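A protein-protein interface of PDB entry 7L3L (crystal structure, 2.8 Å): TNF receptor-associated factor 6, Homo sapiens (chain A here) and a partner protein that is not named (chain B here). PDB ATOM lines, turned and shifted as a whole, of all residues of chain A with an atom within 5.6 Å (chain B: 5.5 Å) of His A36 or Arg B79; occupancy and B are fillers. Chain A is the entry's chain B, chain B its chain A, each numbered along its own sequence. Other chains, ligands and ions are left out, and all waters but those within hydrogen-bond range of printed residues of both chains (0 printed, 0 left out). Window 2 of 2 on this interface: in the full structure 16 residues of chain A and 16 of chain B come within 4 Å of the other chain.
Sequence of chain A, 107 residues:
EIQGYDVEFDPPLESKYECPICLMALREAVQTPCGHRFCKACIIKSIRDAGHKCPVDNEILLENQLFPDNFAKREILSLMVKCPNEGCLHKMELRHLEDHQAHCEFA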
ATOM      1  N   VAL A  30      -1.168  -7.364  22.009  1.00  0.00           N
ATOM      2  CA  VAL A  30      -2.578  -7.009  21.932  1.00  0.00           C
ATOM      3  C   VAL A  30      -2.761  -6.039  20.774  1.00  0.00           C
ATOM      4  O   VAL A  30      -1.832  -5.327  20.386  1.00  0.00           O
ATOM      5  CB  VAL A  30      -3.088  -6.390  23.252  1.00  0.00           C
ATOM      6  CG1 VAL A  30      -2.857  -7.345  24.414  1.00  0.00           C
ATOM      7  CG2 VAL A  30      -2.402  -5.058  23.512  1.00  0.00           C
ATOM      8  N   GLN A  31      -3.970  -6.012  20.219  1.00  0.00           N
ATOM      9  CA  GLN A  31      -4.291  -5.165  19.080  1.00  0.00           C
ATOM     10  C   GLN A  31      -5.417  -4.209  19.447  1.00  0.00           C
ATOM     11  O   GLN A  31      -6.300  -4.542  20.244  1.00  0.00           O
ATOM     12  CB  GLN A  31      -4.694  -6.010  17.859  1.00  0.00           C
ATOM     13  CG  GLN A  31      -4.872  -5.224  16.565  1.00  0.00           C
ATOM     14  CD  GLN A  31      -5.242  -6.109  15.386  1.00  0.00           C
ATOM     15  OE1 GLN A  31      -5.836  -5.649  14.412  1.00  0.00           O
ATOM     16  NE2 GLN A  31      -4.886  -7.384  15.470  1.00  0.00           N
ATOM     17  N   THR A  32      -5.381  -3.011  18.860  1.00  0.00           N
ATOM     18  CA  THR A  32      -6.370  -1.976  19.114  1.00  0.00           C
ATOM     19  C   THR A  32      -7.416  -1.947  18.010  1.00  0.00           C
ATOM     20  O   THR A  32      -7.196  -2.468  16.913  1.00  0.00           O
ATOM     21  CB  THR A  32      -5.695  -0.601  19.215  1.00  0.00           C
ATOM     22  OG1 THR A  32      -5.320  -0.153  17.906  1.00  0.00           O
ATOM     23  CG2 THR A  32      -4.465  -0.665  20.105  1.00  0.00           C
ATOM     24  N   CYS A  34      -8.156   0.464  16.141  1.00  0.00           N
ATOM     25  CA  CYS A  34      -7.621   1.164  14.977  1.00  0.00           C
ATOM     26  C   CYS A  34      -6.554   0.354  14.251  1.00  0.00           C
ATOM     27  O   CYS A  34      -6.095   0.778  13.185  1.00  0.00           O
ATOM     28  CB  CYS A  34      -7.072   2.538  15.366  1.00  0.00           C
ATOM     29  SG  CYS A  34      -6.168   2.576  16.925  1.00  0.00           S
ATOM     30  N   GLY A  35      -6.146  -0.791  14.794  1.00  0.00           N
ATOM     31  CA  GLY A  35      -5.269  -1.693  14.071  1.00  0.00           C
ATOM     32  C   GLY A  35      -3.797  -1.446  14.310  1.00  0.00           C
ATOM     33  O   GLY A  35      -3.029  -1.308  13.356  1.00  0.00           O
ATOM     34  N   HIS A  36      -3.390  -1.390  15.575  1.00  0.00           N
ATOM     35  CA  HIS A  36      -1.991  -1.233  15.935  1.00  0.00           C
ATOM     36  C   HIS A  36      -1.686  -2.179  17.081  1.00  0.00           C
ATOM     37  O   HIS A  36      -2.513  -2.357  17.977  1.00  0.00           O
ATOM     38  CB  HIS A  36      -1.673   0.214  16.322  1.00  0.00           C
ATOM     39  CG  HIS A  36      -1.924   1.197  15.220  1.00  0.00           C
ATOM     40  ND1 HIS A  36      -0.945   1.584  14.332  1.00  0.00           N
ATOM     41  CD2 HIS A  36      -3.048   1.857  14.851  1.00  0.00           C
ATOM     42  CE1 HIS A  36      -1.453   2.445  13.468  1.00  0.00           C
ATOM     43  NE2 HIS A  36      -2.727   2.628  13.762  1.00  0.00           N
ATOM     44  N   ARG A  37      -0.515  -2.802  17.037  1.00  0.00           N
ATOM     45  CA  ARG A  37      -0.125  -3.800  18.021  1.00  0.00           C
ATOM     46  C   ARG A  37       0.825  -3.187  19.041  1.00  0.00           C
ATOM     47  O   ARG A  37       1.691  -2.384  18.692  1.00  0.00           O
ATOM     48  CB  ARG A  37       0.540  -5.000  17.342  1.00  0.00           C
ATOM     49  CG  ARG A  37      -0.262  -5.588  16.185  1.00  0.00           C
ATOM     50  CD  ARG A  37       0.412  -6.835  15.613  1.00  0.00           C
ATOM     51  NE  ARG A  37      -0.431  -7.514  14.628  1.00  0.00           N
ATOM     52  CZ  ARG A  37      -0.235  -7.474  13.314  1.00  0.00           C
ATOM     53  NH1 ARG A  37       0.783  -6.785  12.812  1.00  0.00           N
ATOM     54  NH2 ARG A  37      -1.057  -8.123  12.498  1.00  0.00           N
ATOM     55  N   PHE A  38       0.647  -3.565  20.305  1.00  0.00           N
ATOM     56  CA  PHE A  38       1.529  -3.159  21.389  1.00  0.00           C
ATOM     57  C   PHE A  38       1.759  -4.365  22.287  1.00  0.00           C
ATOM     58  O   PHE A  38       1.100  -5.397  22.154  1.00  0.00           O
ATOM     59  CB  PHE A  38       0.946  -2.004  22.221  1.00  0.00           C
ATOM     60  CG  PHE A  38       0.602  -0.770  21.426  1.00  0.00           C
ATOM     61  CD1 PHE A  38      -0.628  -0.649  20.799  1.00  0.00           C
ATOM     62  CD2 PHE A  38       1.496   0.283  21.338  1.00  0.00           C
ATOM     63  CE1 PHE A  38      -0.951   0.496  20.078  1.00  0.00           C
ATOM     64  CE2 PHE A  38       1.180   1.428  20.621  1.00  0.00           C
ATOM     65  CZ  PHE A  38      -0.044   1.535  19.992  1.00  0.00           C
ATOM     66  N   CYS A  54      -4.809   5.907  21.417  1.00  0.00           N
ATOM     67  CA  CYS A  54      -3.791   5.093  20.769  1.00  0.00           C
ATOM     68  C   CYS A  54      -2.603   5.976  20.418  1.00  0.00           C
ATOM     69  O   CYS A  54      -2.756   6.909  19.618  1.00  0.00           O
ATOM     70  CB  CYS A  54      -4.342   4.425  19.518  1.00  0.00           C
ATOM     71  SG  CYS A  54      -3.117   3.478  18.564  1.00  0.00           S
ATOM     72  N   VAL A  56      -0.218   5.925  18.483  1.00  0.00           N
ATOM     73  CA  VAL A  56       0.213   6.028  17.097  1.00  0.00           C
ATOM     74  C   VAL A  56      -0.708   6.930  16.273  1.00  0.00           C
ATOM     75  O   VAL A  56      -0.245   7.596  15.342  1.00  0.00           O
ATOM     76  CB  VAL A  56       0.324   4.621  16.476  1.00  0.00           C
ATOM     77  CG1 VAL A  56       0.645   4.700  14.990  1.00  0.00           C
ATOM     78  CG2 VAL A  56       1.388   3.810  17.204  1.00  0.00           C
ATOM     79  N   ASP A  57      -2.004   6.992  16.601  1.00  0.00           N
ATOM     80  CA  ASP A  57      -2.942   7.789  15.818  1.00  0.00           C
ATOM     81  C   ASP A  57      -3.902   8.619  16.665  1.00  0.00           C
ATOM     82  O   ASP A  57      -4.825   9.225  16.109  1.00  0.00           O
ATOM     83  CB  ASP A  57      -3.741   6.896  14.858  1.00  0.00           C
ATOM     84  CG  ASP A  57      -4.343   5.687  15.542  1.00  0.00           C
ATOM     85  OD1 ASP A  57      -4.627   5.766  16.754  1.00  0.00           O
ATOM     86  OD2 ASP A  57      -4.541   4.656  14.865  1.00  0.00           O
ATOM     87  N   ASP B  74      -9.607  -8.011  12.756  1.00  0.00           N
ATOM     88  CA  ASP B  74      -8.162  -7.848  12.602  1.00  0.00           C
ATOM     89  C   ASP B  74      -7.891  -6.681  11.654  1.00  0.00           C
ATOM     90  O   ASP B  74      -7.499  -6.840  10.497  1.00  0.00           O
ATOM     91  CB  ASP B  74      -7.523  -9.138  12.113  1.00  0.00           C
ATOM     92  CG  ASP B  74      -6.138  -9.343  12.677  1.00  0.00           C
ATOM     93  OD1 ASP B  74      -5.468  -8.331  12.969  1.00  0.00           O
ATOM     94  OD2 ASP B  74      -5.717 -10.508  12.831  1.00  0.00           O
ATOM     95  N   ASN B  75      -8.123  -5.476  12.186  1.00  0.00           N
ATOM     96  CA  ASN B  75      -7.983  -4.259  11.393  1.00  0.00           C
ATOM     97  C   ASN B  75      -6.529  -3.989  11.022  1.00  0.00           C
ATOM     98  O   ASN B  75      -6.262  -3.310  10.022  1.00  0.00           O
ATOM     99  CB  ASN B  75      -8.570  -3.073  12.156  1.00  0.00           C
ATOM    100  CG  ASN B  75     -10.076  -3.163  12.297  1.00  0.00           C
ATOM    101  OD1 ASN B  75     -10.778  -3.488  11.343  1.00  0.00           O
ATOM    102  ND2 ASN B  75     -10.579  -2.877  13.493  1.00  0.00           N
ATOM    103  N   CYS B  76      -5.582  -4.496  11.818  1.00  0.00           N
ATOM    104  CA  CYS B  76      -4.170  -4.369  11.475  1.00  0.00           C
ATOM    105  C   CYS B  76      -3.798  -5.320  10.348  1.00  0.00           C
ATOM    106  O   CYS B  76      -3.138  -4.929   9.379  1.00  0.00           O
ATOM    107  CB  CYS B  76      -3.307  -4.630  12.709  1.00  0.00           C
ATOM    108  SG  CYS B  76      -1.529  -4.488  12.433  1.00  0.00           S
ATOM    109  N   CYS B  77      -4.206  -6.582  10.463  1.00  0.00           N
ATOM    110  CA  CYS B  77      -4.040  -7.510   9.355  1.00  0.00           C
ATOM    111  C   CYS B  77      -4.812  -7.046   8.133  1.00  0.00           C
ATOM    112  O   CYS B  77      -4.370  -7.267   7.001  1.00  0.00           O
ATOM    113  CB  CYS B  77      -4.495  -8.913   9.761  1.00  0.00           C
ATOM    114  SG  CYS B  77      -4.748 -10.046   8.378  1.00  0.00           S
ATOM    115  N   LYS B  78      -5.959  -6.397   8.340  1.00  0.00           N
ATOM    116  CA  LYS B  78      -6.708  -5.854   7.212  1.00  0.00           C
ATOM    117  C   LYS B  78      -5.880  -4.833   6.446  1.00  0.00           C
ATOM    118  O   LYS B  78      -5.945  -4.770   5.215  1.00  0.00           O
ATOM    119  CB  LYS B  78      -8.017  -5.224   7.691  1.00  0.00           C
ATOM    120  CG  LYS B  78      -8.912  -4.763   6.553  1.00  0.00           C
ATOM    121  CD  LYS B  78     -10.208  -4.139   7.044  1.00  0.00           C
ATOM    122  CE  LYS B  78     -11.104  -3.785   5.869  1.00  0.00           C
ATOM    123  NZ  LYS B  78     -12.352  -3.099   6.287  1.00  0.00           N
ATOM    124  N   ARG B  79      -5.076  -4.040   7.156  1.00  0.00           N
ATOM    125  CA  ARG B  79      -4.280  -3.019   6.483  1.00  0.00           C
ATOM    126  C   ARG B  79      -3.084  -3.621   5.759  1.00  0.00           C
ATOM    127  O   ARG B  79      -2.752  -3.194   4.649  1.00  0.00           O
ATOM    128  CB  ARG B  79      -3.815  -1.963   7.481  1.00  0.00           C
ATOM    129  CG  ARG B  79      -3.407  -0.659   6.824  1.00  0.00           C
ATOM    130  CD  ARG B  79      -3.182   0.427   7.857  1.00  0.00           C
ATOM    131  NE  ARG B  79      -2.553  -0.103   9.061  1.00  0.00           N
ATOM    132  CZ  ARG B  79      -3.130  -0.122  10.256  1.00  0.00           C
ATOM    133  NH1 ARG B  79      -4.355   0.365  10.405  1.00  0.00           N
ATOM    134  NH2 ARG B  79      -2.483  -0.628  11.298  1.00  0.00           N
ATOM    135  N   GLU B  80      -2.423  -4.606   6.370  1.00  0.00           N
ATOM    136  CA  GLU B  80      -1.290  -5.243   5.707  1.00  0.00           C
ATOM    137  C   GLU B  80      -1.717  -5.908   4.404  1.00  0.00           C
ATOM    138  O   GLU B  80      -0.981  -5.879   3.411  1.00  0.00           O
ATOM    139  CB  GLU B  80      -0.639  -6.257   6.645  1.00  0.00           C
ATOM    140  CG  GLU B  80       0.025  -5.620   7.851  1.00  0.00           C
ATOM    141  CD  GLU B  80       0.466  -6.635   8.879  1.00  0.00           C
ATOM    142  OE1 GLU B  80       0.510  -7.839   8.551  1.00  0.00           O
ATOM    143  OE2 GLU B  80       0.771  -6.225  10.018  1.00  0.00           O
ATOM    144  N   VAL B  81      -2.914  -6.497   4.388  1.00  0.00           N
ATOM    145  CA  VAL B  81      -3.418  -7.133   3.176  1.00  0.00           C
ATOM    146  C   VAL B  81      -3.694  -6.088   2.099  1.00  0.00           C
ATOM    147  O   VAL B  81      -3.213  -6.199   0.965  1.00  0.00           O
ATOM    148  CB  VAL B  81      -4.674  -7.963   3.492  1.00  0.00           C
ATOM    149  CG1 VAL B  81      -5.412  -8.306   2.216  1.00  0.00           C
ATOM    150  CG2 VAL B  81      -4.295  -9.228   4.244  1.00  0.00           C
ATOM    151  N   LEU B  82      -4.466  -5.055   2.436  1.00  0.00           N
ATOM    152  CA  LEU B  82      -4.821  -4.044   1.446  1.00  0.00           C
ATOM    153  C   LEU B  82      -3.618  -3.253   0.945  1.00  0.00           C
ATOM    154  O   LEU B  82      -3.752  -2.512  -0.036  1.00  0.00           O
ATOM    155  CB  LEU B  82      -5.875  -3.096   2.021  1.00  0.00           C
ATOM    156  CG  LEU B  82      -7.208  -3.747   2.397  1.00  0.00           C
ATOM    157  CD1 LEU B  82      -7.868  -2.999   3.543  1.00  0.00           C
ATOM    158  CD2 LEU B  82      -8.136  -3.828   1.193  1.00  0.00           C
ATOM    159  N   ASN B  83      -2.457  -3.391   1.582  1.00  0.00           N
ATOM    160  CA  ASN B  83      -1.225  -2.776   1.111  1.00  0.00           C
ATOM    161  C   ASN B  83      -0.375  -3.728   0.280  1.00  0.00           C
ATOM    162  O   ASN B  83       0.745  -3.369  -0.098  1.00  0.00           O
ATOM    163  CB  ASN B  83      -0.409  -2.251   2.297  1.00  0.00           C
ATOM    164  CG  ASN B  83      -0.893  -0.900   2.789  1.00  0.00           C
ATOM    165  OD1 ASN B  83      -1.309  -0.053   2.000  1.00  0.00           O
ATOM    166  ND2 ASN B  83      -0.843  -0.696   4.099  1.00  0.00           N
ATOM    167  N   LEU B  84      -0.873  -4.928  -0.004  1.00  0.00           N
ATOM    168  CA  LEU B  84      -0.160  -5.848  -0.878  1.00  0.00           C
ATOM    169  C   LEU B  84      -0.263  -5.391  -2.329  1.00  0.00           C
ATOM    170  O   LEU B  84      -1.311  -4.912  -2.776  1.00  0.00           O
ATOM    171  CB  LEU B  84      -0.720  -7.264  -0.734  1.00  0.00           C
ATOM    172  CG  LEU B  84      -0.573  -7.935   0.633  1.00  0.00           C
ATOM    173  CD1 LEU B  84      -1.122  -9.351   0.592  1.00  0.00           C
ATOM    174  CD2 LEU B  84       0.879  -7.924   1.083  1.00  0.00           C
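Among the printed residues, pairs that only touch across the chains: His A36 with Arg B79.
Hydrophobic or aromatic side chains of chain A that line the printed part of chain B: His A36.
Printed residues of chain B that touch a printed residue of chain A: Asp B74, Asn B75, Cys B76, Arg B79 and Glu B80.
Among the printed residues, 9 pairs touch across the chains.
The side-chain carboxylate of Asp B74 lies within hydrogen-bond range of the backbone NH of Cys B77, at 3.3 Å.
The side-chain amide nitrogen (ND2) of Asn B83 is in hydrogen-bond range of the backbone carbonyl oxygen (O) of Arg B79 (3.2 Å).
OG1 of Thr A32 lies close to N of Cys A34, 3.4 Å away.
The side-chain sulfur (SG) of Cys B76 sits at hydrogen-bond distance from the side-chain carboxylate (OE2) of Glu B80 (3.8 Å).
The side-chain hydroxyl (OG1) of Thr A32 is in hydrogen-bond range of the backbone NH (N) of His A36.
OG1 of Thr A32 lies within hydrogen-bond range of N of Gly A35, 3.3 Å away.
Of chain B, only Arg B79 (3.9 Å) comes within 4 Å of His A36.
Arg B79 touches three residues of chain A.
Printed residues of chain A within 4 Å of Asn B75: Gln A31.
Of the printed residues of chain B, Gly A35 touches Cys B76 (3.4 Å) and Arg B79 (2.2 Å).
Of the printed residues of chain B, Gln A31 touches Asp B74, Asn B75 and Cys B76.
Of the printed residues of chain A, Cys B76 touches Gln A31, Gly A35 and Arg A37.
Asn B83 touches none of the printed residues of chain A.
Val A56 touches none of the printed residues of chain B.
The nearest residue of chain B that does not touch His A36 is Cys B76 (4.3 Å).
NH2 of Arg B79 lies close to O of Gly A35 (2.2 Å).
OE1 of Gln A31 lies within hydrogen-bond range of N of Asn B75 (3.2 Å).
The side-chain amide nitrogen of Gln A31 lies within hydrogen-bond range of the side-chain carboxylate of Asp B74, at 2.7 Å.
The backbone carbonyl oxygen (O) of Gly A35 lies close to the side-chain sulfur (SG) of Cys B76 (3.6 Å).
OE1 of Gln A31 sits at hydrogen-bond distance from N of Cys B76.
NH1 of Arg A37 lies within hydrogen-bond range of SG of Cys B76, 3.3 Å away.
The side-chain carboxylate (OE2) of Glu B80 is in salt-bridge range of the guanidinium group (NH1) of Arg A37 (2.8 Å).
The backbone carbonyl oxygen (O) of Cys A34 lies within hydrogen-bond range of the guanidinium group (NH1) of Arg B79 (3.3 Å).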
